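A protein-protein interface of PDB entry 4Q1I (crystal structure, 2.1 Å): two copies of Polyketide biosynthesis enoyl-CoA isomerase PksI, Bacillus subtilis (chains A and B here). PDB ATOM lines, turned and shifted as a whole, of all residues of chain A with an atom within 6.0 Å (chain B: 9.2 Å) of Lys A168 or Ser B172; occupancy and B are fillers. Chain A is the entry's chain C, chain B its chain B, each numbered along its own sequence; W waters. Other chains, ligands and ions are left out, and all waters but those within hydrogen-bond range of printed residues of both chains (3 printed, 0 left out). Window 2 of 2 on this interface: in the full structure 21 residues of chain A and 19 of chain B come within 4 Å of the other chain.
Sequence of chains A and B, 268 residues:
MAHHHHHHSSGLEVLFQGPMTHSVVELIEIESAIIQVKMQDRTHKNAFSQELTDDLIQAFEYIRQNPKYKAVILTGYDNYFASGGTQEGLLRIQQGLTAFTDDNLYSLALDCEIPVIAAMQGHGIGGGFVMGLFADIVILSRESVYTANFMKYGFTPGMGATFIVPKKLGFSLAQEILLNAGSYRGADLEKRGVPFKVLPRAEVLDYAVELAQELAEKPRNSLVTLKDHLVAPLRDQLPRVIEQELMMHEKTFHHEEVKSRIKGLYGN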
ATOM      1  N   GLY A 132      15.539   9.516  15.374  1.00  0.00           N
ATOM      2  CA  GLY A 132      14.054   9.271  15.419  1.00  0.00           C
ATOM      3  C   GLY A 132      13.265  10.586  15.407  1.00  0.00           C
ATOM      4  O   GLY A 132      12.203  10.692  14.708  1.00  0.00           O
ATOM      5  N   LEU A 133      13.773  11.632  16.119  1.00  0.00           N
ATOM      6  CA  LEU A 133      13.030  12.893  16.156  1.00  0.00           C
ATOM      7  C   LEU A 133      12.994  13.631  14.795  1.00  0.00           C
ATOM      8  O   LEU A 133      12.258  14.589  14.651  1.00  0.00           O
ATOM      9  CB  LEU A 133      13.534  13.844  17.274  1.00  0.00           C
ATOM     10  CG  LEU A 133      13.480  13.260  18.702  1.00  0.00           C
ATOM     11  CD1 LEU A 133      14.119  14.126  19.789  1.00  0.00           C
ATOM     12  CD2 LEU A 133      12.030  12.883  19.051  1.00  0.00           C
ATOM     13  N   PHE A 134      13.798  13.208  13.827  1.00  0.00           N
ATOM     14  CA  PHE A 134      13.773  13.811  12.509  1.00  0.00           C
ATOM     15  C   PHE A 134      12.712  13.183  11.599  1.00  0.00           C
ATOM     16  O   PHE A 134      12.460  13.673  10.494  1.00  0.00           O
ATOM     17  CB  PHE A 134      15.182  13.846  11.858  1.00  0.00           C
ATOM     18  CG  PHE A 134      16.039  15.036  12.355  1.00  0.00           C
ATOM     19  CD1 PHE A 134      16.004  16.303  11.680  1.00  0.00           C
ATOM     20  CD2 PHE A 134      16.890  14.888  13.465  1.00  0.00           C
ATOM     21  CE1 PHE A 134      16.782  17.383  12.175  1.00  0.00           C
ATOM     22  CE2 PHE A 134      17.664  15.981  13.929  1.00  0.00           C
ATOM     23  CZ  PHE A 134      17.612  17.222  13.276  1.00  0.00           C
ATOM     24  N   ALA A 135      12.084  12.113  12.077  1.00  0.00           N
ATOM     25  CA  ALA A 135      10.996  11.527  11.297  1.00  0.00           C
ATOM     26  C   ALA A 135       9.771  12.408  11.447  1.00  0.00           C
ATOM     27  O   ALA A 135       9.680  13.229  12.383  1.00  0.00           O
ATOM     28  CB  ALA A 135      10.733  10.100  11.721  1.00  0.00           C
ATOM     29  N   ASP A 136       8.824  12.229  10.544  1.00  0.00           N
ATOM     30  CA  ASP A 136       7.579  13.013  10.558  1.00  0.00           C
ATOM     31  C   ASP A 136       6.654  12.574  11.695  1.00  0.00           C
ATOM     32  O   ASP A 136       5.991  13.405  12.297  1.00  0.00           O
ATOM     33  CB  ASP A 136       6.866  12.853   9.217  1.00  0.00           C
ATOM     34  CG  ASP A 136       7.738  13.305   8.089  1.00  0.00           C
ATOM     35  OD1 ASP A 136       7.617  14.468   7.667  1.00  0.00           O
ATOM     36  OD2 ASP A 136       8.561  12.506   7.635  1.00  0.00           O
ATOM     37  N   ILE A 137       6.650  11.278  12.000  1.00  0.00           N
ATOM     38  CA  ILE A 137       5.829  10.776  13.091  1.00  0.00           C
ATOM     39  C   ILE A 137       6.749   9.927  13.928  1.00  0.00           C
ATOM     40  O   ILE A 137       7.609   9.196  13.414  1.00  0.00           O
ATOM     41  CB  ILE A 137       4.743   9.879  12.513  1.00  0.00           C
ATOM     42  CG1 ILE A 137       4.028  10.653  11.405  1.00  0.00           C
ATOM     43  CG2 ILE A 137       3.868   9.153  13.596  1.00  0.00           C
ATOM     44  CD1 ILE A 137       2.769  11.292  11.795  1.00  0.00           C
ATOM     45  N   VAL A 138       6.577  10.039  15.217  1.00  0.00           N
ATOM     46  CA  VAL A 138       7.512   9.423  16.143  1.00  0.00           C
ATOM     47  C   VAL A 138       6.620   8.536  17.054  1.00  0.00           C
ATOM     48  O   VAL A 138       5.595   9.022  17.568  1.00  0.00           O
ATOM     49  CB  VAL A 138       8.241  10.439  17.012  1.00  0.00           C
ATOM     50  CG1 VAL A 138       9.029   9.664  18.132  1.00  0.00           C
ATOM     51  CG2 VAL A 138       9.229  11.350  16.211  1.00  0.00           C
ATOM     52  N   PHE A 163      18.719  21.553  18.467  1.00  0.00           N
ATOM     53  CA  PHE A 163      17.842  22.045  17.406  1.00  0.00           C
ATOM     54  C   PHE A 163      16.486  21.345  17.411  1.00  0.00           C
ATOM     55  O   PHE A 163      15.455  21.954  17.560  1.00  0.00           O
ATOM     56  CB  PHE A 163      18.542  21.705  16.093  1.00  0.00           C
ATOM     57  CG  PHE A 163      17.763  22.056  14.865  1.00  0.00           C
ATOM     58  CD1 PHE A 163      17.675  23.376  14.435  1.00  0.00           C
ATOM     59  CD2 PHE A 163      17.164  21.055  14.091  1.00  0.00           C
ATOM     60  CE1 PHE A 163      16.980  23.713  13.258  1.00  0.00           C
ATOM     61  CE2 PHE A 163      16.476  21.392  12.907  1.00  0.00           C
ATOM     62  CZ  PHE A 163      16.397  22.721  12.484  1.00  0.00           C
ATOM     63  N   ILE A 164      16.495  20.043  17.258  1.00  0.00           N
ATOM     64  CA  ILE A 164      15.292  19.269  16.991  1.00  0.00           C
ATOM     65  C   ILE A 164      14.434  18.906  18.257  1.00  0.00           C
ATOM     66  O   ILE A 164      13.193  18.762  18.169  1.00  0.00           O
ATOM     67  CB  ILE A 164      15.618  17.964  16.235  1.00  0.00           C
ATOM     68  CG1 ILE A 164      14.330  17.437  15.602  1.00  0.00           C
ATOM     69  CG2 ILE A 164      16.080  16.810  17.151  1.00  0.00           C
ATOM     70  CD1 ILE A 164      13.908  18.271  14.404  1.00  0.00           C
ATOM     71  N   VAL A 165      15.083  18.746  19.422  1.00  0.00           N
ATOM     72  CA  VAL A 165      14.376  18.429  20.654  1.00  0.00           C
ATOM     73  C   VAL A 165      13.326  19.463  21.088  1.00  0.00           C
ATOM     74  O   VAL A 165      12.171  19.110  21.312  1.00  0.00           O
ATOM     75  CB  VAL A 165      15.346  18.047  21.813  1.00  0.00           C
ATOM     76  CG1 VAL A 165      14.553  17.692  23.060  1.00  0.00           C
ATOM     77  CG2 VAL A 165      16.199  16.861  21.390  1.00  0.00           C
ATOM     78  N   PRO A 166      13.702  20.752  21.194  1.00  0.00           N
ATOM     79  CA  PRO A 166      12.633  21.681  21.545  1.00  0.00           C
ATOM     80  C   PRO A 166      11.510  21.759  20.488  1.00  0.00           C
ATOM     81  O   PRO A 166      10.296  21.940  20.836  1.00  0.00           O
ATOM     82  CB  PRO A 166      13.356  23.058  21.711  1.00  0.00           C
ATOM     83  CG  PRO A 166      14.834  22.736  21.751  1.00  0.00           C
ATOM     84  CD  PRO A 166      15.004  21.446  20.949  1.00  0.00           C
ATOM     85  N   LYS A 167      11.868  21.548  19.227  1.00  0.00           N
ATOM     86  CA  LYS A 167      10.879  21.707  18.162  1.00  0.00           C
ATOM     87  C   LYS A 167       9.870  20.522  18.201  1.00  0.00           C
ATOM     88  O   LYS A 167       8.695  20.728  17.933  1.00  0.00           O
ATOM     89  CB  LYS A 167      11.572  21.822  16.819  1.00  0.00           C
ATOM     90  CG  LYS A 167      12.379  23.137  16.735  1.00  0.00           C
ATOM     91  CD  LYS A 167      13.518  23.034  15.721  1.00  0.00           C
ATOM     92  CE  LYS A 167      14.492  24.210  15.889  1.00  0.00           C
ATOM     93  NZ  LYS A 167      14.076  25.225  14.905  1.00  0.00           N
ATOM     94  N   LYS A 168      10.341  19.320  18.521  1.00  0.00           N
ATOM     95  CA  LYS A 168       9.446  18.151  18.567  1.00  0.00           C
ATOM     96  C   LYS A 168       8.782  17.861  19.896  1.00  0.00           C
ATOM     97  O   LYS A 168       7.684  17.278  19.917  1.00  0.00           O
ATOM     98  CB  LYS A 168      10.253  16.911  18.104  1.00  0.00           C
ATOM     99  CG  LYS A 168      10.282  16.873  16.578  1.00  0.00           C
ATOM    100  CD  LYS A 168       9.397  15.717  16.156  1.00  0.00           C
ATOM    101  CE  LYS A 168       8.630  16.083  14.926  1.00  0.00           C
ATOM    102  NZ  LYS A 168       8.723  15.159  13.804  1.00  0.00           N
ATOM    103  N   LEU A 169       9.443  18.261  21.015  1.00  0.00           N
ATOM    104  CA  LEU A 169       9.017  17.961  22.377  1.00  0.00           C
ATOM    105  C   LEU A 169       8.544  19.231  23.069  1.00  0.00           C
ATOM    106  O   LEU A 169       7.920  19.188  24.139  1.00  0.00           O
ATOM    107  CB  LEU A 169      10.173  17.281  23.175  1.00  0.00           C
ATOM    108  CG  LEU A 169      10.146  15.811  22.835  1.00  0.00           C
ATOM    109  CD1 LEU A 169      11.069  14.954  23.698  1.00  0.00           C
ATOM    110  CD2 LEU A 169       8.685  15.403  23.024  1.00  0.00           C
ATOM    111  N   GLY A 170       8.830  20.372  22.468  1.00  0.00           N
ATOM    112  CA  GLY A 170       8.361  21.585  23.034  1.00  0.00           C
ATOM    113  C   GLY A 170       9.521  22.110  23.904  1.00  0.00           C
ATOM    114  O   GLY A 170      10.302  21.374  24.515  1.00  0.00           O
ATOM    115  N   PRO A 195       3.821  14.537  22.713  1.00  0.00           N
ATOM    116  CA  PRO A 195       2.833  14.381  21.616  1.00  0.00           C
ATOM    117  C   PRO A 195       2.858  13.012  20.860  1.00  0.00           C
ATOM    118  O   PRO A 195       1.977  12.743  19.975  1.00  0.00           O
ATOM    119  CB  PRO A 195       3.267  15.472  20.599  1.00  0.00           C
ATOM    120  CG  PRO A 195       4.748  15.748  20.872  1.00  0.00           C
ATOM    121  CD  PRO A 195       4.864  15.551  22.385  1.00  0.00           C
ATOM    122  N   PHE A 196       3.840  12.172  21.177  1.00  0.00           N
ATOM    123  CA  PHE A 196       3.997  10.855  20.559  1.00  0.00           C
ATOM    124  C   PHE A 196       3.076   9.812  21.154  1.00  0.00           C
ATOM    125  O   PHE A 196       2.826   9.756  22.377  1.00  0.00           O
ATOM    126  CB  PHE A 196       5.442  10.356  20.763  1.00  0.00           C
ATOM    127  CG  PHE A 196       6.479  11.407  20.473  1.00  0.00           C
ATOM    128  CD1 PHE A 196       6.282  12.365  19.453  1.00  0.00           C
ATOM    129  CD2 PHE A 196       7.653  11.442  21.211  1.00  0.00           C
ATOM    130  CE1 PHE A 196       7.264  13.280  19.136  1.00  0.00           C
ATOM    131  CE2 PHE A 196       8.622  12.404  20.936  1.00  0.00           C
ATOM    132  CZ  PHE A 196       8.428  13.341  19.885  1.00  0.00           C
ATOM    133  N   VAL B 165      -3.178  24.803  13.541  1.00  0.00           N
ATOM    134  CA  VAL B 165      -3.142  23.500  14.202  1.00  0.00           C
ATOM    135  C   VAL B 165      -1.778  23.310  14.951  1.00  0.00           C
ATOM    136  O   VAL B 165      -1.777  22.969  16.114  1.00  0.00           O
ATOM    137  CB  VAL B 165      -3.428  22.328  13.236  1.00  0.00           C
ATOM    138  CG1 VAL B 165      -3.332  20.950  13.971  1.00  0.00           C
ATOM    139  CG2 VAL B 165      -4.830  22.441  12.625  1.00  0.00           C
ATOM    140  N   PRO B 166      -0.603  23.554  14.289  1.00  0.00           N
ATOM    141  CA  PRO B 166       0.614  23.500  15.096  1.00  0.00           C
ATOM    142  C   PRO B 166       0.688  24.549  16.173  1.00  0.00           C
ATOM    143  O   PRO B 166       1.298  24.285  17.216  1.00  0.00           O
ATOM    144  CB  PRO B 166       1.758  23.812  14.096  1.00  0.00           C
ATOM    145  CG  PRO B 166       1.118  23.823  12.760  1.00  0.00           C
ATOM    146  CD  PRO B 166      -0.324  23.582  12.834  1.00  0.00           C
ATOM    147  N   LYS B 167       0.138  25.734  15.890  1.00  0.00           N
ATOM    148  CA  LYS B 167       0.154  26.811  16.890  1.00  0.00           C
ATOM    149  C   LYS B 167      -0.656  26.389  18.161  1.00  0.00           C
ATOM    150  O   LYS B 167      -0.291  26.704  19.238  1.00  0.00           O
ATOM    151  CB  LYS B 167      -0.467  28.081  16.291  1.00  0.00           C
ATOM    152  CG  LYS B 167      -0.286  29.252  17.287  1.00  0.00           C
ATOM    153  CD  LYS B 167       1.227  29.625  17.342  1.00  0.00           C
ATOM    154  CE  LYS B 167       1.533  30.896  18.147  1.00  0.00           C
ATOM    155  NZ  LYS B 167       3.013  31.141  18.189  1.00  0.00           N
ATOM    156  N   LEU B 169      -1.893  23.066  18.922  1.00  0.00           N
ATOM    157  CA  LEU B 169      -1.720  21.697  19.402  1.00  0.00           C
ATOM    158  C   LEU B 169      -0.263  21.284  19.380  1.00  0.00           C
ATOM    159  O   LEU B 169       0.071  20.239  19.858  1.00  0.00           O
ATOM    160  CB  LEU B 169      -2.563  20.721  18.578  1.00  0.00           C
ATOM    161  CG  LEU B 169      -4.071  20.949  18.661  1.00  0.00           C
ATOM    162  CD1 LEU B 169      -4.924  19.929  17.877  1.00  0.00           C
ATOM    163  CD2 LEU B 169      -4.461  20.971  20.119  1.00  0.00           C
ATOM    164  N   GLY B 170       0.618  22.100  18.833  1.00  0.00           N
ATOM    165  CA  GLY B 170       2.086  21.803  18.846  1.00  0.00           C
ATOM    166  C   GLY B 170       2.422  21.204  17.483  1.00  0.00           C
ATOM    167  O   GLY B 170       1.564  20.515  16.861  1.00  0.00           O
ATOM    168  N   PHE B 171       3.648  21.404  17.043  1.00  0.00           N
ATOM    169  CA  PHE B 171       4.100  20.974  15.742  1.00  0.00           C
ATOM    170  C   PHE B 171       3.987  19.403  15.511  1.00  0.00           C
ATOM    171  O   PHE B 171       3.428  18.899  14.488  1.00  0.00           O
ATOM    172  CB  PHE B 171       5.594  21.495  15.508  1.00  0.00           C
ATOM    173  CG  PHE B 171       6.210  20.999  14.168  1.00  0.00           C
ATOM    174  CD1 PHE B 171       5.825  21.575  12.973  1.00  0.00           C
ATOM    175  CD2 PHE B 171       7.148  19.929  14.105  1.00  0.00           C
ATOM    176  CE1 PHE B 171       6.398  21.169  11.745  1.00  0.00           C
ATOM    177  CE2 PHE B 171       7.682  19.503  12.871  1.00  0.00           C
ATOM    178  CZ  PHE B 171       7.296  20.128  11.684  1.00  0.00           C
ATOM    179  N   SER B 172       4.487  18.619  16.467  1.00  0.00           N
ATOM    180  CA  SER B 172       4.470  17.174  16.311  1.00  0.00           C
ATOM    181  C   SER B 172       3.118  16.594  16.078  1.00  0.00           C
ATOM    182  O   SER B 172       2.938  15.750  15.193  1.00  0.00           O
ATOM    183  CB  SER B 172       5.095  16.495  17.508  1.00  0.00           C
ATOM    184  OG  SER B 172       6.461  16.791  17.492  1.00  0.00           O
ATOM    185  N   LEU B 173       2.152  16.950  16.940  1.00  0.00           N
ATOM    186  CA  LEU B 173       0.837  16.379  16.851  1.00  0.00           C
ATOM    187  C   LEU B 173       0.153  16.881  15.591  1.00  0.00           C
ATOM    188  O   LEU B 173      -0.566  16.133  14.882  1.00  0.00           O
ATOM    189  CB  LEU B 173      -0.038  16.679  18.076  1.00  0.00           C
ATOM    190  CG  LEU B 173      -1.407  16.036  18.049  1.00  0.00           C
ATOM    191  CD1 LEU B 173      -1.392  14.482  17.749  1.00  0.00           C
ATOM    192  CD2 LEU B 173      -2.278  16.372  19.276  1.00  0.00           C
ATOM    193  N   ALA B 174       0.393  18.150  15.288  1.00  0.00           N
ATOM    194  CA  ALA B 174      -0.158  18.733  14.035  1.00  0.00           C
ATOM    195  C   ALA B 174       0.315  17.980  12.752  1.00  0.00           C
ATOM    196  O   ALA B 174      -0.516  17.745  11.823  1.00  0.00           O
ATOM    197  CB  ALA B 174       0.230  20.265  13.995  1.00  0.00           C
ATOM    198  N   GLN B 175       1.554  17.492  12.707  1.00  0.00           N
ATOM    199  CA  GLN B 175       2.007  16.723  11.505  1.00  0.00           C
ATOM    200  C   GLN B 175       1.103  15.509  11.276  1.00  0.00           C
ATOM    201  O   GLN B 175       0.680  15.215  10.173  1.00  0.00           O
ATOM    202  CB  GLN B 175       3.441  16.207  11.638  1.00  0.00           C
ATOM    203  CG  GLN B 175       4.420  17.369  11.505  1.00  0.00           C
ATOM    204  CD  GLN B 175       5.825  16.964  11.770  1.00  0.00           C
ATOM    205  OE1 GLN B 175       6.257  16.924  12.943  1.00  0.00           O
ATOM    206  NE2 GLN B 175       6.619  16.699  10.648  1.00  0.00           N
ATOM    207  N   GLU B 176       0.814  14.815  12.348  1.00  0.00           N
ATOM    208  CA  GLU B 176      -0.034  13.605  12.298  1.00  0.00           C
ATOM    209  C   GLU B 176      -1.452  14.001  11.893  1.00  0.00           C
ATOM    210  O   GLU B 176      -2.042  13.381  11.043  1.00  0.00           O
ATOM    211  CB  GLU B 176      -0.069  12.997  13.722  1.00  0.00           C
ATOM    212  CG  GLU B 176      -1.029  11.814  13.739  1.00  0.00           C
ATOM    213  CD  GLU B 176      -1.175  11.152  15.079  1.00  0.00           C
ATOM    214  OE1 GLU B 176      -0.172  10.870  15.752  1.00  0.00           O
ATOM    215  OE2 GLU B 176      -2.335  10.937  15.453  1.00  0.00           O
ATOM    216  N   ILE B 177      -2.023  15.024  12.545  1.00  0.00           N
ATOM    217  CA  ILE B 177      -3.383  15.493  12.255  1.00  0.00           C
ATOM    218  C   ILE B 177      -3.558  15.902  10.763  1.00  0.00           C
ATOM    219  O   ILE B 177      -4.560  15.517  10.125  1.00  0.00           O
ATOM    220  CB  ILE B 177      -3.784  16.686  13.234  1.00  0.00           C
ATOM    221  CG1 ILE B 177      -3.968  16.153  14.696  1.00  0.00           C
ATOM    222  CG2 ILE B 177      -5.008  17.450  12.738  1.00  0.00           C
ATOM    223  CD1 ILE B 177      -4.235  17.179  15.798  1.00  0.00           C
ATOM    224  N   LEU B 178      -2.602  16.685  10.243  1.00  0.00           N
ATOM    225  CA  LEU B 178      -2.622  17.335   8.934  1.00  0.00           C
ATOM    226  C   LEU B 178      -2.259  16.309   7.821  1.00  0.00           C
ATOM    227  O   LEU B 178      -3.033  16.191   6.836  1.00  0.00           O
ATOM    228  CB  LEU B 178      -1.605  18.500   8.857  1.00  0.00           C
ATOM    229  CG  LEU B 178      -2.104  19.648   9.740  1.00  0.00           C
ATOM    230  CD1 LEU B 178      -0.992  20.697   9.939  1.00  0.00           C
ATOM    231  CD2 LEU B 178      -3.443  20.226   9.251  1.00  0.00           C
ATOM    232  N   LEU B 179      -1.180  15.524   8.013  1.00  0.00           N
ATOM    233  CA  LEU B 179      -0.755  14.544   6.977  1.00  0.00           C
ATOM    234  C   LEU B 179      -1.774  13.410   6.800  1.00  0.00           C
ATOM    235  O   LEU B 179      -2.058  13.053   5.685  1.00  0.00           O
ATOM    236  CB  LEU B 179       0.585  13.888   7.253  1.00  0.00           C
ATOM    237  CG  LEU B 179       1.863  14.710   7.028  1.00  0.00           C
ATOM    238  CD1 LEU B 179       3.008  14.027   7.771  1.00  0.00           C
ATOM    239  CD2 LEU B 179       2.142  14.905   5.541  1.00  0.00           C
ATOM    240  N   TYR B 184     -10.517  11.676  15.365  1.00  0.00           N
ATOM    241  CA  TYR B 184     -10.274  11.532  16.784  1.00  0.00           C
ATOM    242  C   TYR B 184     -11.518  11.869  17.608  1.00  0.00           C
ATOM    243  O   TYR B 184     -12.177  12.820  17.320  1.00  0.00           O
ATOM    244  CB  TYR B 184      -9.166  12.467  17.237  1.00  0.00           C
ATOM    245  CG  TYR B 184      -7.881  12.405  16.476  1.00  0.00           C
ATOM    246  CD1 TYR B 184      -6.810  11.737  16.980  1.00  0.00           C
ATOM    247  CD2 TYR B 184      -7.738  13.018  15.243  1.00  0.00           C
ATOM    248  CE1 TYR B 184      -5.633  11.666  16.294  1.00  0.00           C
ATOM    249  CE2 TYR B 184      -6.563  12.943  14.542  1.00  0.00           C
ATOM    250  CZ  TYR B 184      -5.511  12.276  15.067  1.00  0.00           C
ATOM    251  OH  TYR B 184      -4.362  12.222  14.401  1.00  0.00           O
ATOM    252  N   ARG B 192      -4.072  12.156  24.119  1.00  0.00           N
ATOM    253  CA  ARG B 192      -2.785  12.543  23.531  1.00  0.00           C
ATOM    254  C   ARG B 192      -2.198  13.792  24.197  1.00  0.00           C
ATOM    255  O   ARG B 192      -1.072  14.160  23.918  1.00  0.00           O
ATOM    256  CB  ARG B 192      -2.920  12.786  22.017  1.00  0.00           C
ATOM    257  CG  ARG B 192      -3.390  11.535  21.319  1.00  0.00           C
ATOM    258  CD  ARG B 192      -2.324  10.432  21.257  1.00  0.00           C
ATOM    259  NE  ARG B 192      -1.155  10.893  20.479  1.00  0.00           N
ATOM    260  CZ  ARG B 192      -1.030  10.746  19.160  1.00  0.00           C
ATOM    261  NH1 ARG B 192      -2.018  10.172  18.431  1.00  0.00           N
ATOM    262  NH2 ARG B 192       0.085  11.174  18.584  1.00  0.00           N
HETATM  263  O   HOH W   1       5.891  16.595   7.918  1.00  0.00           O
HETATM  264  O   HOH W   2       0.396  11.712  22.751  1.00  0.00           O
HETATM  265  O   HOH W   3       5.755  19.898  19.004  1.00  0.00           O
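OG of Ser B172 lies within hydrogen-bond range of O of Lys A168.
The side-chain amino group of Lys A168 is in hydrogen-bond range of the side-chain amide oxygen of Gln B175 (3.2 Å).
The backbone carbonyl oxygen (O) of Pro A195 sits at hydrogen-bond distance from the guanidinium group (NH2) of Arg B192, at 2.8 Å.
The side-chain hydroxyl of Tyr B184 lies within hydrogen-bond range of the side-chain carboxylate of Glu B176.
The side-chain carboxylate (OE1) of Glu B176 lies within salt-bridge range of the guanidinium group (NH2) of Arg B192 (2.9 Å).
The backbone carbonyl oxygen (O) of Ala A135 sits at hydrogen-bond distance from the side-chain amino group (NZ) of Lys A168 (2.6 Å).
5 positions are printed for both chains.
Of the 7 pairs that touch across the chains among the printed residues, none has its exchanged pair printed and touching as well.
Gly A132 touches none of the printed residues of chain B.
Printed residues of chain B within 4 Å of Asp A136: Gln B175 (3.6 Å).
Lys A168 touches just these residues of chain B: Ser B172 and Gln B175.
Ala B174 touches none of the printed residues of chain A.
Of the printed residues of chain A, Gln B175 touches Asp A136 and Lys A168.
Printed residues of chain A within 4 Å of Glu B176: Ile A137 (3.7 Å).
The nearest residue of chain A that does not touch Ser B172 is Lys A167 (4.5 Å).
Gln B175 touches Asp A136.
Ile A137 touches Glu B176 (CD1 to CA, 3.7 Å).
Pro A195 touches Ser B172.
Phe A196 touches Ser B172.
Water W1 bridges OD1 of Asp A136 and NE2 of Gln B175.
Water W2 lies within hydrogen-bond range of NE of Arg B192 (2.9 Å), O of Phe A196 (3.1 Å) and O of Pro A195 (3.4 Å).
Water W3 lies within hydrogen-bond range of the backbone NH of Ser B172 (3.1 Å), the backbone carbonyl oxygen of Lys A167 (3.2 Å), the backbone NH of Phe B171 (3.2 Å) and the backbone carbonyl oxygen of Lys A168 (3.4 Å).
Hydrophobic or aromatic side chains of chain A that line the printed part of chain B: Ile A137, Pro A195 and Phe A196.
Among the printed residues, 7 pairs touch across the chains.
Among the printed residues, no Asp or Glu carboxylate lies within 4 Å of a Lys or Arg side-chain nitrogen of the other chain.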
